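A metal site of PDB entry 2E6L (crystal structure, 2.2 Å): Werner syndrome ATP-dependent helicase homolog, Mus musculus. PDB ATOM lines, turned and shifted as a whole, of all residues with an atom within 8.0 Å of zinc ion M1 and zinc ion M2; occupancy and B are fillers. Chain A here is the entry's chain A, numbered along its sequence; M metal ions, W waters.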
ATOM      1  N   PHE A  45      18.815  25.714  -7.840  1.00  0.00           N
ATOM      2  CA  PHE A  45      19.616  24.744  -8.584  1.00  0.00           C
ATOM      3  C   PHE A  45      20.966  24.470  -7.933  1.00  0.00           C
ATOM      4  O   PHE A  45      21.601  25.367  -7.369  1.00  0.00           O
ATOM      5  CB  PHE A  45      19.816  25.258 -10.021  1.00  0.00           C
ATOM      6  CG  PHE A  45      20.743  24.419 -10.869  1.00  0.00           C
ATOM      7  CD1 PHE A  45      22.133  24.501 -10.704  1.00  0.00           C
ATOM      8  CD2 PHE A  45      20.232  23.549 -11.827  1.00  0.00           C
ATOM      9  CE1 PHE A  45      22.985  23.733 -11.499  1.00  0.00           C
ATOM     10  CE2 PHE A  45      21.072  22.774 -12.621  1.00  0.00           C
ATOM     11  CZ  PHE A  45      22.452  22.874 -12.458  1.00  0.00           C
ATOM     12  N   ASP A  46      21.409  23.217  -8.012  1.00  0.00           N
ATOM     13  CA  ASP A  46      22.692  22.805  -7.456  1.00  0.00           C
ATOM     14  C   ASP A  46      23.048  21.408  -7.972  1.00  0.00           C
ATOM     15  O   ASP A  46      22.187  20.711  -8.536  1.00  0.00           O
ATOM     16  CB  ASP A  46      22.629  22.816  -5.928  1.00  0.00           C
ATOM     17  CG  ASP A  46      23.974  22.559  -5.302  1.00  0.00           C
ATOM     18  OD1 ASP A  46      24.969  23.124  -5.804  1.00  0.00           O
ATOM     19  OD2 ASP A  46      24.028  21.828  -4.301  1.00  0.00           O
ATOM     20  N   MET A  47      24.301  21.011  -7.810  1.00  0.00           N
ATOM     21  CA  MET A  47      24.766  19.698  -8.277  1.00  0.00           C
ATOM     22  C   MET A  47      25.775  19.105  -7.310  1.00  0.00           C
ATOM     23  O   MET A  47      26.422  19.829  -6.553  1.00  0.00           O
ATOM     24  CB  MET A  47      25.427  19.799  -9.661  1.00  0.00           C
ATOM     25  CG  MET A  47      24.646  20.578 -10.721  1.00  0.00           C
ATOM     26  SD  MET A  47      25.402  20.434 -12.374  1.00  0.00           S
ATOM     27  CE  MET A  47      27.119  20.746 -11.992  1.00  0.00           C
ATOM     28  N   GLU A  48      25.917  17.781  -7.346  1.00  0.00           N
ATOM     29  CA  GLU A  48      26.878  17.105  -6.484  1.00  0.00           C
ATOM     30  C   GLU A  48      27.622  16.062  -7.312  1.00  0.00           C
ATOM     31  O   GLU A  48      27.145  15.639  -8.362  1.00  0.00           O
ATOM     32  CB  GLU A  48      26.193  16.387  -5.319  1.00  0.00           C
ATOM     33  CG  GLU A  48      25.215  17.207  -4.501  1.00  0.00           C
ATOM     34  CD  GLU A  48      25.839  18.408  -3.807  1.00  0.00           C
ATOM     35  OE1 GLU A  48      27.048  18.352  -3.454  1.00  0.00           O
ATOM     36  OE2 GLU A  48      25.111  19.395  -3.596  1.00  0.00           O
ATOM     37  N   TRP A  49      28.790  15.651  -6.825  1.00  0.00           N
ATOM     38  CA  TRP A  49      29.582  14.638  -7.511  1.00  0.00           C
ATOM     39  C   TRP A  49      30.651  14.134  -6.541  1.00  0.00           C
ATOM     40  O   TRP A  49      31.113  14.876  -5.686  1.00  0.00           O
ATOM     41  CB  TRP A  49      30.234  15.215  -8.772  1.00  0.00           C
ATOM     42  CG  TRP A  49      31.069  16.435  -8.536  1.00  0.00           C
ATOM     43  CD1 TRP A  49      32.382  16.471  -8.149  1.00  0.00           C
ATOM     44  CD2 TRP A  49      30.644  17.797  -8.655  1.00  0.00           C
ATOM     45  NE1 TRP A  49      32.803  17.770  -8.015  1.00  0.00           N
ATOM     46  CE2 TRP A  49      31.763  18.610  -8.317  1.00  0.00           C
ATOM     47  CE3 TRP A  49      29.445  18.414  -9.001  1.00  0.00           C
ATOM     48  CZ2 TRP A  49      31.700  20.004  -8.319  1.00  0.00           C
ATOM     49  CZ3 TRP A  49      29.375  19.804  -9.009  1.00  0.00           C
ATOM     50  CH2 TRP A  49      30.500  20.586  -8.673  1.00  0.00           C
ATOM     51  N   VAL A  63      24.647  14.040  -9.195  1.00  0.00           N
ATOM     52  CA  VAL A  63      23.308  14.493  -8.827  1.00  0.00           C
ATOM     53  C   VAL A  63      22.998  15.919  -9.275  1.00  0.00           C
ATOM     54  O   VAL A  63      23.863  16.789  -9.242  1.00  0.00           O
ATOM     55  CB  VAL A  63      23.104  14.419  -7.296  1.00  0.00           C
ATOM     56  CG1 VAL A  63      21.650  14.765  -6.937  1.00  0.00           C
ATOM     57  CG2 VAL A  63      23.466  13.041  -6.773  1.00  0.00           C
ATOM     58  N   GLN A  65      20.080  18.859  -8.561  1.00  0.00           N
ATOM     59  CA  GLN A  65      18.950  19.242  -7.708  1.00  0.00           C
ATOM     60  C   GLN A  65      18.206  20.457  -8.232  1.00  0.00           C
ATOM     61  O   GLN A  65      18.817  21.460  -8.625  1.00  0.00           O
ATOM     62  CB  GLN A  65      19.435  19.546  -6.280  1.00  0.00           C
ATOM     63  CG  GLN A  65      20.273  18.450  -5.647  1.00  0.00           C
ATOM     64  CD  GLN A  65      21.764  18.766  -5.666  1.00  0.00           C
ATOM     65  OE1 GLN A  65      22.277  19.481  -4.782  1.00  0.00           O
ATOM     66  NE2 GLN A  65      22.463  18.254  -6.671  1.00  0.00           N
ATOM     67  N   GLY A 101      21.665  29.775  -7.980  1.00  0.00           N
ATOM     68  CA  GLY A 101      22.627  29.022  -7.198  1.00  0.00           C
ATOM     69  C   GLY A 101      23.887  29.822  -6.912  1.00  0.00           C
ATOM     70  O   GLY A 101      23.997  30.986  -7.299  1.00  0.00           O
ATOM     71  N   VAL A 102      24.810  29.185  -6.218  1.00  0.00           N
ATOM     72  CA  VAL A 102      26.091  29.792  -5.851  1.00  0.00           C
ATOM     73  C   VAL A 102      27.191  28.994  -6.539  1.00  0.00           C
ATOM     74  O   VAL A 102      27.252  27.774  -6.407  1.00  0.00           O
ATOM     75  CB  VAL A 102      26.278  29.750  -4.320  1.00  0.00           C
ATOM     76  CG1 VAL A 102      27.703  30.148  -3.952  1.00  0.00           C
ATOM     77  CG2 VAL A 102      25.280  30.687  -3.663  1.00  0.00           C
ATOM     78  N   GLY A 103      28.070  29.686  -7.268  1.00  0.00           N
ATOM     79  CA  GLY A 103      29.132  29.003  -7.980  1.00  0.00           C
ATOM     80  C   GLY A 103      28.491  28.215  -9.100  1.00  0.00           C
ATOM     81  O   GLY A 103      28.993  27.175  -9.536  1.00  0.00           O
ATOM     82  N   ILE A 104      27.363  28.739  -9.580  1.00  0.00           N
ATOM     83  CA  ILE A 104      26.594  28.085 -10.633  1.00  0.00           C
ATOM     84  C   ILE A 104      27.206  28.148 -12.036  1.00  0.00           C
ATOM     85  O   ILE A 104      26.871  27.324 -12.894  1.00  0.00           O
ATOM     86  CB  ILE A 104      25.140  28.646 -10.647  1.00  0.00           C
ATOM     87  CG1 ILE A 104      24.249  27.748 -11.522  1.00  0.00           C
ATOM     88  CG2 ILE A 104      25.141  30.092 -11.131  1.00  0.00           C
ATOM     89  CD1 ILE A 104      22.793  28.165 -11.497  1.00  0.00           C
ATOM     90  N   ASP A 107      29.064  25.197 -12.334  1.00  0.00           N
ATOM     91  CA  ASP A 107      28.186  24.046 -12.571  1.00  0.00           C
ATOM     92  C   ASP A 107      27.898  23.948 -14.070  1.00  0.00           C
ATOM     93  O   ASP A 107      27.960  22.867 -14.644  1.00  0.00           O
ATOM     94  CB  ASP A 107      26.856  24.188 -11.821  1.00  0.00           C
ATOM     95  CG  ASP A 107      27.003  24.010 -10.315  1.00  0.00           C
ATOM     96  OD1 ASP A 107      27.832  23.191  -9.872  1.00  0.00           O
ATOM     97  OD2 ASP A 107      26.262  24.683  -9.563  1.00  0.00           O
ATOM     98  N   LEU A 141      28.283  29.243  -0.167  1.00  0.00           N
ATOM     99  CA  LEU A 141      26.832  29.163  -0.061  1.00  0.00           C
ATOM    100  C   LEU A 141      26.422  29.292   1.409  1.00  0.00           C
ATOM    101  O   LEU A 141      25.477  30.001   1.747  1.00  0.00           O
ATOM    102  CB  LEU A 141      26.318  27.829  -0.635  1.00  0.00           C
ATOM    103  CG  LEU A 141      24.803  27.615  -0.696  1.00  0.00           C
ATOM    104  CD1 LEU A 141      24.237  27.405   0.692  1.00  0.00           C
ATOM    105  CD2 LEU A 141      24.128  28.792  -1.355  1.00  0.00           C
ATOM    106  N   LEU A 153      24.149  26.074   7.647  1.00  0.00           N
ATOM    107  CA  LEU A 153      24.057  24.880   6.809  1.00  0.00           C
ATOM    108  C   LEU A 153      25.009  23.777   7.283  1.00  0.00           C
ATOM    109  O   LEU A 153      26.165  24.041   7.601  1.00  0.00           O
ATOM    110  CB  LEU A 153      24.401  25.228   5.359  1.00  0.00           C
ATOM    111  CG  LEU A 153      23.368  24.923   4.290  1.00  0.00           C
ATOM    112  CD1 LEU A 153      22.076  25.682   4.554  1.00  0.00           C
ATOM    113  CD2 LEU A 153      23.937  25.298   2.932  1.00  0.00           C
ATOM    114  N   ARG A 160      28.979  16.275   2.682  1.00  0.00           N
ATOM    115  CA  ARG A 160      29.353  17.159   1.587  1.00  0.00           C
ATOM    116  C   ARG A 160      30.302  16.485   0.595  1.00  0.00           C
ATOM    117  O   ARG A 160      30.173  16.674  -0.619  1.00  0.00           O
ATOM    118  CB  ARG A 160      30.014  18.422   2.160  1.00  0.00           C
ATOM    119  CG  ARG A 160      30.320  19.493   1.125  1.00  0.00           C
ATOM    120  CD  ARG A 160      30.716  20.814   1.810  1.00  0.00           C
ATOM    121  NE  ARG A 160      32.155  20.930   2.044  1.00  0.00           N
ATOM    122  CZ  ARG A 160      32.851  20.171   2.884  1.00  0.00           C
ATOM    123  NH1 ARG A 160      32.264  19.219   3.584  1.00  0.00           N
ATOM    124  NH2 ARG A 160      34.156  20.364   3.016  1.00  0.00           N
ATOM    125  N   TRP A 164      28.750  10.591  -3.909  1.00  0.00           N
ATOM    126  CA  TRP A 164      27.454  10.888  -4.503  1.00  0.00           C
ATOM    127  C   TRP A 164      27.025   9.970  -5.640  1.00  0.00           C
ATOM    128  O   TRP A 164      25.873  10.011  -6.081  1.00  0.00           O
ATOM    129  CB  TRP A 164      27.411  12.349  -4.964  1.00  0.00           C
ATOM    130  CG  TRP A 164      27.468  13.324  -3.828  1.00  0.00           C
ATOM    131  CD1 TRP A 164      28.581  13.971  -3.347  1.00  0.00           C
ATOM    132  CD2 TRP A 164      26.377  13.737  -2.991  1.00  0.00           C
ATOM    133  NE1 TRP A 164      28.237  14.754  -2.270  1.00  0.00           N
ATOM    134  CE2 TRP A 164      26.897  14.625  -2.021  1.00  0.00           C
ATOM    135  CE3 TRP A 164      25.010  13.429  -2.969  1.00  0.00           C
ATOM    136  CZ2 TRP A 164      26.098  15.217  -1.043  1.00  0.00           C
ATOM    137  CZ3 TRP A 164      24.211  14.021  -1.991  1.00  0.00           C
ATOM    138  CH2 TRP A 164      24.753  14.906  -1.044  1.00  0.00           C
ATOM    139  N   TYR A 176      20.699  16.867   2.430  1.00  0.00           N
ATOM    140  CA  TYR A 176      21.763  17.831   2.202  1.00  0.00           C
ATOM    141  C   TYR A 176      21.691  18.364   0.775  1.00  0.00           C
ATOM    142  O   TYR A 176      21.757  19.569   0.542  1.00  0.00           O
ATOM    143  CB  TYR A 176      23.135  17.189   2.452  1.00  0.00           C
ATOM    144  CG  TYR A 176      24.302  18.030   1.991  1.00  0.00           C
ATOM    145  CD1 TYR A 176      24.667  18.062   0.641  1.00  0.00           C
ATOM    146  CD2 TYR A 176      25.019  18.808   2.899  1.00  0.00           C
ATOM    147  CE1 TYR A 176      25.731  18.864   0.210  1.00  0.00           C
ATOM    148  CE2 TYR A 176      26.078  19.619   2.466  1.00  0.00           C
ATOM    149  CZ  TYR A 176      26.423  19.630   1.121  1.00  0.00           C
ATOM    150  OH  TYR A 176      27.461  20.419   0.694  1.00  0.00           O
ATOM    151  N   ALA A 177      21.556  17.471  -0.195  1.00  0.00           N
ATOM    152  CA  ALA A 177      21.462  17.882  -1.593  1.00  0.00           C
ATOM    153  C   ALA A 177      20.230  18.745  -1.825  1.00  0.00           C
ATOM    154  O   ALA A 177      20.299  19.758  -2.530  1.00  0.00           O
ATOM    155  CB  ALA A 177      21.421  16.660  -2.502  1.00  0.00           C
ATOM    156  N   ALA A 178      19.100  18.372  -1.222  1.00  0.00           N
ATOM    157  CA  ALA A 178      17.869  19.142  -1.389  1.00  0.00           C
ATOM    158  C   ALA A 178      17.997  20.523  -0.743  1.00  0.00           C
ATOM    159  O   ALA A 178      17.530  21.528  -1.282  1.00  0.00           O
ATOM    160  CB  ALA A 178      16.676  18.395  -0.798  1.00  0.00           C
ATOM    161  N   THR A 179      18.621  20.562   0.431  1.00  0.00           N
ATOM    162  CA  THR A 179      18.785  21.811   1.146  1.00  0.00           C
ATOM    163  C   THR A 179      19.692  22.810   0.399  1.00  0.00           C
ATOM    164  O   THR A 179      19.444  24.013   0.443  1.00  0.00           O
ATOM    165  CB  THR A 179      19.292  21.528   2.583  1.00  0.00           C
ATOM    166  OG1 THR A 179      18.318  20.724   3.267  1.00  0.00           O
ATOM    167  CG2 THR A 179      19.478  22.819   3.362  1.00  0.00           C
ATOM    168  N   ASP A 180      20.727  22.320  -0.284  1.00  0.00           N
ATOM    169  CA  ASP A 180      21.602  23.222  -1.041  1.00  0.00           C
ATOM    170  C   ASP A 180      20.834  23.918  -2.174  1.00  0.00           C
ATOM    171  O   ASP A 180      21.042  25.105  -2.422  1.00  0.00           O
ATOM    172  CB  ASP A 180      22.806  22.469  -1.630  1.00  0.00           C
ATOM    173  CG  ASP A 180      24.061  22.559  -0.744  1.00  0.00           C
ATOM    174  OD1 ASP A 180      25.141  22.132  -1.204  1.00  0.00           O
ATOM    175  OD2 ASP A 180      23.956  23.045   0.406  1.00  0.00           O
ATOM    176  N   ALA A 181      19.960  23.179  -2.846  1.00  0.00           N
ATOM    177  CA  ALA A 181      19.148  23.757  -3.927  1.00  0.00           C
ATOM    178  C   ALA A 181      18.105  24.685  -3.330  1.00  0.00           C
ATOM    179  O   ALA A 181      17.813  25.759  -3.865  1.00  0.00           O
ATOM    180  CB  ALA A 181      18.461  22.635  -4.723  1.00  0.00           C
HETATM  181 ZN    ZN M   1      25.649  21.263  -3.012  1.00  0.00          ZN
HETATM  182 ZN    ZN M   2      26.969  23.847  -5.570  1.00  0.00          ZN
HETATM  183  O   HOH W   1      28.047  20.628  -2.061  1.00  0.00           O
HETATM  184  O   HOH W   2      26.258  25.317  -3.910  1.00  0.00           O
HETATM  185  O   HOH W   3      27.549  22.198  -4.028  1.00  0.00           O
HETATM  186  O   HOH W   4      27.464  22.234  -6.931  1.00  0.00           O
HETATM  187  O   HOH W   5      29.313  23.686  -5.131  1.00  0.00           O
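OH of Tyr 176 sits close to OD1 of Asp 180 (3.5 Å). The backbone NH (N) of Glu 48 is in hydrogen-bond range of the backbone carbonyl oxygen (O) of Val 63, 3.0 Å away. N of Gln 65 sits at hydrogen-bond distance from O of Asp 46 (2.8 Å). The side-chain amide oxygen (OE1) of Gln 65 lies close to the side-chain carboxylate (OE2) of Glu 48 (3.1 Å).
Merely in contact with zinc ion M1: Met 47. Within 4 Å of zinc ion M1: Asp 46, Met 47, Glu 48 and Asp 180.
Of the 22 residues printed, 1 comes within 4 Å of zinc ion M2. The nearest printed residue that does not touch zinc ion M2 is Val 102 (4.03 Å).
Zinc ion M1 is bound by the side-chain carboxylate of Glu 48 (2.0 Å), the side-chain carboxylate of Asp 180 (2.1 Å), the side-chain carboxylate of Asp 46 (2.1 Å) and water W3 (2.3 Å). Zinc ion M1 has four donor atoms within binding distance. Slightly farther from zinc ion M1 lies water W1 (2.7 Å).
Zinc ion M2 is bound by the side-chain carboxylate of Asp 46 (2.1 Å), water W4 (2.2 Å), water W2 (2.3 Å), water W3 (2.3 Å) and water W5 (2.4 Å). Zinc ion M2 has five donor atoms within binding distance.
Water W1 lies within hydrogen-bond range of the side-chain hydroxyl of Tyr 176 and the side-chain carboxylate of Glu 48. Water W4 bridges O of Met 47 (2.6 Å) and OD1 of Asp 107 (3.1 Å).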
